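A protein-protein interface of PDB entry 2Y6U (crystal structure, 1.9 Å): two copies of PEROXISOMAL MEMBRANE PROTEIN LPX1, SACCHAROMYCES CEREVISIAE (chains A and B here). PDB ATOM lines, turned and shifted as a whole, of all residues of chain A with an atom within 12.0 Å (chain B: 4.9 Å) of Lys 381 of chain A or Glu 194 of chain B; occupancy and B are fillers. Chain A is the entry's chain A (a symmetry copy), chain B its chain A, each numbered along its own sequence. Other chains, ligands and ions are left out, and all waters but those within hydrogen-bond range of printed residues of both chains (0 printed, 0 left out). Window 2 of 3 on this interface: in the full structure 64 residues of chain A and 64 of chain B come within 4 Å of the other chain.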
ATOM      1  N   PHE A 371     -16.598   0.105  27.855  1.00  0.00           N
ATOM      2  CA  PHE A 371     -17.706   0.549  27.039  1.00  0.00           C
ATOM      3  C   PHE A 371     -18.982  -0.184  27.422  1.00  0.00           C
ATOM      4  O   PHE A 371     -20.009   0.458  27.575  1.00  0.00           O
ATOM      5  CB  PHE A 371     -17.471   0.349  25.565  1.00  0.00           C
ATOM      6  CG  PHE A 371     -18.622   0.780  24.724  1.00  0.00           C
ATOM      7  CD1 PHE A 371     -18.786   2.114  24.399  1.00  0.00           C
ATOM      8  CD2 PHE A 371     -19.549  -0.143  24.243  1.00  0.00           C
ATOM      9  CE1 PHE A 371     -19.811   2.500  23.614  1.00  0.00           C
ATOM     10  CE2 PHE A 371     -20.618   0.258  23.453  1.00  0.00           C
ATOM     11  CZ  PHE A 371     -20.767   1.579  23.161  1.00  0.00           C
ATOM     12  N   ASP A 372     -18.942  -1.489  27.583  1.00  0.00           N
ATOM     13  CA  ASP A 372     -20.153  -2.230  27.971  1.00  0.00           C
ATOM     14  C   ASP A 372     -20.723  -1.708  29.294  1.00  0.00           C
ATOM     15  O   ASP A 372     -21.942  -1.552  29.435  1.00  0.00           O
ATOM     16  CB  ASP A 372     -19.870  -3.734  28.103  1.00  0.00           C
ATOM     17  CG  ASP A 372     -19.690  -4.438  26.738  1.00  0.00           C
ATOM     18  OD1 ASP A 372     -20.138  -3.881  25.683  1.00  0.00           O
ATOM     19  OD2 ASP A 372     -19.111  -5.571  26.744  1.00  0.00           O
ATOM     20  N   SER A 373     -19.860  -1.466  30.270  1.00  0.00           N
ATOM     21  CA  SER A 373     -20.253  -0.946  31.573  1.00  0.00           C
ATOM     22  C   SER A 373     -20.916   0.433  31.434  1.00  0.00           C
ATOM     23  O   SER A 373     -21.973   0.737  31.994  1.00  0.00           O
ATOM     24  CB  SER A 373     -18.981  -0.819  32.437  1.00  0.00           C
ATOM     25  OG  SER A 373     -19.278  -0.393  33.750  1.00  0.00           O
ATOM     26  N   PHE A 374     -20.264   1.296  30.680  1.00  0.00           N
ATOM     27  CA  PHE A 374     -20.743   2.670  30.493  1.00  0.00           C
ATOM     28  C   PHE A 374     -22.088   2.670  29.779  1.00  0.00           C
ATOM     29  O   PHE A 374     -23.032   3.389  30.198  1.00  0.00           O
ATOM     30  CB  PHE A 374     -19.663   3.477  29.728  1.00  0.00           C
ATOM     31  CG  PHE A 374     -20.060   4.888  29.400  1.00  0.00           C
ATOM     32  CD1 PHE A 374     -20.098   5.840  30.349  1.00  0.00           C
ATOM     33  CD2 PHE A 374     -20.402   5.230  28.119  1.00  0.00           C
ATOM     34  CE1 PHE A 374     -20.473   7.118  30.010  1.00  0.00           C
ATOM     35  CE2 PHE A 374     -20.752   6.475  27.784  1.00  0.00           C
ATOM     36  CZ  PHE A 374     -20.785   7.427  28.700  1.00  0.00           C
ATOM     37  N   LYS A 375     -22.208   1.858  28.722  1.00  0.00           N
ATOM     38  CA  LYS A 375     -23.460   1.735  27.975  1.00  0.00           C
ATOM     39  C   LYS A 375     -24.591   1.336  28.960  1.00  0.00           C
ATOM     40  O   LYS A 375     -25.695   1.949  28.954  1.00  0.00           O
ATOM     41  CB  LYS A 375     -23.322   0.717  26.837  1.00  0.00           C
ATOM     42  CG  LYS A 375     -24.651   0.394  26.143  1.00  0.00           C
ATOM     43  CD  LYS A 375     -24.617  -0.910  25.305  1.00  0.00           C
ATOM     44  CE  LYS A 375     -24.434  -2.167  26.134  1.00  0.00           C
ATOM     45  NZ  LYS A 375     -25.365  -3.264  25.686  1.00  0.00           N
ATOM     46  N   ASN A 376     -24.327   0.332  29.802  1.00  0.00           N
ATOM     47  CA  ASN A 376     -25.354  -0.100  30.786  1.00  0.00           C
ATOM     48  C   ASN A 376     -25.712   1.007  31.780  1.00  0.00           C
ATOM     49  O   ASN A 376     -26.859   1.105  32.207  1.00  0.00           O
ATOM     50  CB  ASN A 376     -24.926  -1.401  31.478  1.00  0.00           C
ATOM     51  CG  ASN A 376     -24.847  -2.615  30.482  1.00  0.00           C
ATOM     52  OD1 ASN A 376     -25.529  -2.651  29.435  1.00  0.00           O
ATOM     53  ND2 ASN A 376     -23.993  -3.589  30.813  1.00  0.00           N
ATOM     54  N   GLU A 377     -24.757   1.848  32.164  1.00  0.00           N
ATOM     55  CA  GLU A 377     -25.115   2.932  33.056  1.00  0.00           C
ATOM     56  C   GLU A 377     -25.865   4.073  32.273  1.00  0.00           C
ATOM     57  O   GLU A 377     -26.761   4.706  32.824  1.00  0.00           O
ATOM     58  CB  GLU A 377     -23.901   3.428  33.862  1.00  0.00           C
ATOM     59  CG  GLU A 377     -22.888   2.326  34.410  1.00  0.00           C
ATOM     60  CD  GLU A 377     -23.495   1.056  35.077  1.00  0.00           C
ATOM     61  OE1 GLU A 377     -24.624   1.129  35.614  1.00  0.00           O
ATOM     62  OE2 GLU A 377     -22.811  -0.022  35.101  1.00  0.00           O
ATOM     63  N   ALA A 378     -25.552   4.291  31.006  1.00  0.00           N
ATOM     64  CA  ALA A 378     -26.158   5.405  30.271  1.00  0.00           C
ATOM     65  C   ALA A 378     -27.496   5.101  29.582  1.00  0.00           C
ATOM     66  O   ALA A 378     -28.300   6.002  29.309  1.00  0.00           O
ATOM     67  CB  ALA A 378     -25.154   5.962  29.215  1.00  0.00           C
ATOM     68  N   LEU A 379     -27.721   3.843  29.233  1.00  0.00           N
ATOM     69  CA  LEU A 379     -28.848   3.534  28.399  1.00  0.00           C
ATOM     70  C   LEU A 379     -30.123   3.663  29.256  1.00  0.00           C
ATOM     71  O   LEU A 379     -30.195   3.120  30.353  1.00  0.00           O
ATOM     72  CB  LEU A 379     -28.667   2.136  27.845  1.00  0.00           C
ATOM     73  CG  LEU A 379     -29.229   1.829  26.484  1.00  0.00           C
ATOM     74  CD1 LEU A 379     -28.387   0.769  25.847  1.00  0.00           C
ATOM     75  CD2 LEU A 379     -30.627   1.291  26.766  1.00  0.00           C
ATOM     76  N   VAL A 380     -31.094   4.451  28.775  1.00  0.00           N
ATOM     77  CA  VAL A 380     -32.378   4.607  29.463  1.00  0.00           C
ATOM     78  C   VAL A 380     -33.332   3.649  28.742  1.00  0.00           C
ATOM     79  O   VAL A 380     -33.731   3.895  27.599  1.00  0.00           O
ATOM     80  CB  VAL A 380     -32.855   6.093  29.438  1.00  0.00           C
ATOM     81  CG1 VAL A 380     -34.299   6.238  29.989  1.00  0.00           C
ATOM     82  CG2 VAL A 380     -31.854   6.989  30.222  1.00  0.00           C
ATOM     83  N   LYS A 381     -33.693   2.560  29.415  1.00  0.00           N
ATOM     84  CA  LYS A 381     -34.388   1.417  28.759  1.00  0.00           C
ATOM     85  C   LYS A 381     -35.878   1.609  28.430  1.00  0.00           C
ATOM     86  O   LYS A 381     -36.477   2.661  28.689  1.00  0.00           O
ATOM     87  CB  LYS A 381     -34.207   0.145  29.596  1.00  0.00           C
ATOM     88  CG  LYS A 381     -32.752  -0.332  29.673  1.00  0.00           C
ATOM     89  CD  LYS A 381     -32.636  -1.833  30.044  1.00  0.00           C
ATOM     90  CE  LYS A 381     -31.185  -2.252  30.361  1.00  0.00           C
ATOM     91  NZ  LYS A 381     -31.182  -3.604  30.992  1.00  0.00           N
ATOM     92  N   GLY B 179     -37.984   7.567  30.133  1.00  0.00           N
ATOM     93  CA  GLY B 179     -37.798   6.097  30.218  1.00  0.00           C
ATOM     94  C   GLY B 179     -37.308   5.650  31.597  1.00  0.00           C
ATOM     95  O   GLY B 179     -37.143   6.479  32.498  1.00  0.00           O
ATOM     96  N   ALA B 180     -37.058   4.347  31.763  1.00  0.00           N
ATOM     97  CA  ALA B 180     -36.762   3.769  33.098  1.00  0.00           C
ATOM     98  C   ALA B 180     -35.641   2.694  33.057  1.00  0.00           C
ATOM     99  O   ALA B 180     -35.956   1.500  33.152  1.00  0.00           O
ATOM    100  CB  ALA B 180     -38.060   3.176  33.701  1.00  0.00           C
ATOM    101  N   GLY B 181     -34.343   3.072  32.990  1.00  0.00           N
ATOM    102  CA  GLY B 181     -33.788   4.379  33.427  1.00  0.00           C
ATOM    103  C   GLY B 181     -33.095   4.158  34.778  1.00  0.00           C
ATOM    104  O   GLY B 181     -33.735   3.715  35.748  1.00  0.00           O
ATOM    105  N   ILE B 192     -28.615   8.093  27.290  1.00  0.00           N
ATOM    106  CA  ILE B 192     -29.044   8.034  25.927  1.00  0.00           C
ATOM    107  C   ILE B 192     -30.314   7.153  25.909  1.00  0.00           C
ATOM    108  O   ILE B 192     -30.335   6.163  26.600  1.00  0.00           O
ATOM    109  CB  ILE B 192     -27.983   7.431  24.983  1.00  0.00           C
ATOM    110  CG1 ILE B 192     -28.430   7.631  23.539  1.00  0.00           C
ATOM    111  CG2 ILE B 192     -27.749   5.927  25.270  1.00  0.00           C
ATOM    112  CD1 ILE B 192     -27.359   7.362  22.408  1.00  0.00           C
ATOM    113  N   PRO B 193     -31.346   7.518  25.111  1.00  0.00           N
ATOM    114  CA  PRO B 193     -32.505   6.613  25.046  1.00  0.00           C
ATOM    115  C   PRO B 193     -32.144   5.373  24.228  1.00  0.00           C
ATOM    116  O   PRO B 193     -31.415   5.476  23.248  1.00  0.00           O
ATOM    117  CB  PRO B 193     -33.631   7.457  24.377  1.00  0.00           C
ATOM    118  CG  PRO B 193     -33.159   8.702  24.103  1.00  0.00           C
ATOM    119  CD  PRO B 193     -31.652   8.845  24.536  1.00  0.00           C
ATOM    120  N   GLU B 194     -32.625   4.232  24.662  1.00  0.00           N
ATOM    121  CA  GLU B 194     -32.354   2.945  24.041  1.00  0.00           C
ATOM    122  C   GLU B 194     -32.687   2.919  22.563  1.00  0.00           C
ATOM    123  O   GLU B 194     -31.874   2.441  21.754  1.00  0.00           O
ATOM    124  CB  GLU B 194     -33.107   1.847  24.775  1.00  0.00           C
ATOM    125  CG  GLU B 194     -32.865   0.436  24.253  1.00  0.00           C
ATOM    126  CD  GLU B 194     -33.504  -0.643  25.109  1.00  0.00           C
ATOM    127  OE1 GLU B 194     -34.284  -0.345  26.063  1.00  0.00           O
ATOM    128  OE2 GLU B 194     -33.217  -1.822  24.806  1.00  0.00           O
ATOM    129  N   ASN B 195     -33.876   3.400  22.191  1.00  0.00           N
ATOM    130  CA  ASN B 195     -34.267   3.440  20.761  1.00  0.00           C
ATOM    131  C   ASN B 195     -33.239   4.234  19.916  1.00  0.00           C
ATOM    132  O   ASN B 195     -32.877   3.816  18.819  1.00  0.00           O
ATOM    133  CB  ASN B 195     -35.671   4.048  20.559  1.00  0.00           C
ATOM    134  CG  ASN B 195     -36.796   3.145  21.037  1.00  0.00           C
ATOM    135  OD1 ASN B 195     -36.625   1.938  21.249  1.00  0.00           O
ATOM    136  ND2 ASN B 195     -37.980   3.732  21.181  1.00  0.00           N
ATOM    137  N   LEU B 196     -32.773   5.367  20.414  1.00  0.00           N
ATOM    138  CA  LEU B 196     -31.750   6.136  19.689  1.00  0.00           C
ATOM    139  C   LEU B 196     -30.442   5.335  19.560  1.00  0.00           C
ATOM    140  O   LEU B 196     -29.833   5.338  18.500  1.00  0.00           O
ATOM    141  CB  LEU B 196     -31.461   7.526  20.323  1.00  0.00           C
ATOM    142  CG  LEU B 196     -30.396   8.398  19.623  1.00  0.00           C
ATOM    143  CD1 LEU B 196     -30.802   8.697  18.139  1.00  0.00           C
ATOM    144  CD2 LEU B 196     -29.956   9.721  20.371  1.00  0.00           C
ATOM    145  N   TYR B 197     -29.986   4.710  20.644  1.00  0.00           N
ATOM    146  CA  TYR B 197     -28.747   3.898  20.639  1.00  0.00           C
ATOM    147  C   TYR B 197     -28.786   2.797  19.568  1.00  0.00           C
ATOM    148  O   TYR B 197     -27.866   2.650  18.764  1.00  0.00           O
ATOM    149  CB  TYR B 197     -28.551   3.226  21.999  1.00  0.00           C
ATOM    150  CG  TYR B 197     -27.293   2.375  22.076  1.00  0.00           C
ATOM    151  CD1 TYR B 197     -26.054   2.961  22.404  1.00  0.00           C
ATOM    152  CD2 TYR B 197     -27.326   0.997  21.807  1.00  0.00           C
ATOM    153  CE1 TYR B 197     -24.893   2.196  22.497  1.00  0.00           C
ATOM    154  CE2 TYR B 197     -26.164   0.225  21.881  1.00  0.00           C
ATOM    155  CZ  TYR B 197     -24.926   0.864  22.219  1.00  0.00           C
ATOM    156  OH  TYR B 197     -23.759   0.116  22.293  1.00  0.00           O
ATOM    157  N   ASN B 198     -29.879   2.031  19.594  1.00  0.00           N
ATOM    158  CA  ASN B 198     -30.079   0.875  18.718  1.00  0.00           C
ATOM    159  C   ASN B 198     -30.034   1.290  17.253  1.00  0.00           C
ATOM    160  O   ASN B 198     -29.414   0.624  16.416  1.00  0.00           O
ATOM    161  CB  ASN B 198     -31.395   0.149  19.035  1.00  0.00           C
ATOM    162  CG  ASN B 198     -31.324  -0.698  20.309  1.00  0.00           C
ATOM    163  OD1 ASN B 198     -30.234  -1.035  20.790  1.00  0.00           O
ATOM    164  ND2 ASN B 198     -32.501  -1.098  20.828  1.00  0.00           N
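The backbone carbonyl oxygen (O) of Val 380 of chain A lies within hydrogen-bond range of the backbone NH (N) of Glu 194 of chain B, 3.2 Å away.
N of Ile 192 of chain B is in hydrogen-bond range of O of Ala 378 of chain A, at 2.9 Å.
N of Val 380 of chain A is in hydrogen-bond range of O of Ile 192 of chain B (2.9 Å).
Among the printed residues, pairs that only touch across the chains: Lys 381 of chain A with Glu 194 of chain B (3.2 Å), Leu 379 of chain A with Glu 194 of chain B (3.2 Å), Lys 375 of chain A with Tyr 197 of chain B (3.3 Å), Phe 371 of chain A with Tyr 197 of chain B (3.4 Å), Val 380 of chain A with Gly 179 of chain B (3.5 Å), Leu 379 of chain A with Ile 192 of chain B (3.5 Å), Lys 381 of chain A with Ala 180 of chain B (3.6 Å), Lys 381 of chain A with Gly 181 of chain B (3.7 Å), Val 380 of chain A with Ala 180 of chain B (3.8 Å), Val 380 of chain A with Pro 193 of chain B (3.9 Å), Val 380 of chain A with Gly 181 of chain B (3.9 Å) and Lys 381 of chain A with Gly 179 of chain B (3.99 Å).
Of the printed residues of chain B, Lys 381 of chain A touches Gly 179 (3.99 Å), Ala 180 (3.6 Å), Gly 181 (3.7 Å) and Glu 194 (3.2 Å).
Of chain A, only Leu 379, Val 380 and Lys 381 come within 4 Å of Glu 194 of chain B.
Of chain A, only Val 380 and Lys 381 come within 4 Å of Gly 181 of chain B.
Of the printed residues of chain A, Ile 192 of chain B touches Ala 378 (2.9 Å), Leu 379 (3.5 Å) and Val 380 (2.9 Å).
Of the printed residues of chain A, Pro 193 of chain B touches Val 380 (3.9 Å).
No residue of chain A comes within 4 Å of Asn 198 of chain B.
Of the printed residues of chain A, Gly 179 of chain B touches Val 380 (3.5 Å) and Lys 381 (3.99 Å).
Of the printed residues of chain B, Leu 379 of chain A touches Ile 192 and Glu 194.
Asn 376 of chain A touches none of the printed residues of chain B.
Asn 195 of chain B touches none of the printed residues of chain A.
The nearest printed residue of chain B that does not touch Lys 381 of chain A is Ile 192 of chain B (5.7 Å).
The nearest residue of chain A that does not touch Glu 194 of chain B is Ala 378 of chain A (6.6 Å).
Of the 10 printed residues of chain B, 7 touch a printed residue of chain A.
Hydrophobic or aromatic side chains of chain B within 4 Å of the printed part of chain A: Tyr 197.
Printed residues of chain A that touch a printed residue of chain B: Phe 371, Lys 375, Ala 378, Leu 379, Val 380 and Lys 381.
Hydrophobic or aromatic side chains of chain A within 4 Å of the printed part of chain B: Phe 371, Leu 379 and Val 380.
Among the printed residues, 15 pairs touch across the chains.
Among the printed residues, no Asp or Glu carboxylate lies within 4 Å of a Lys or Arg side-chain nitrogen of the other chain.
No position is printed for both chains.
Of the 15 pairs that touch across the chains among the printed residues, none has its exchanged pair printed and touching as well.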
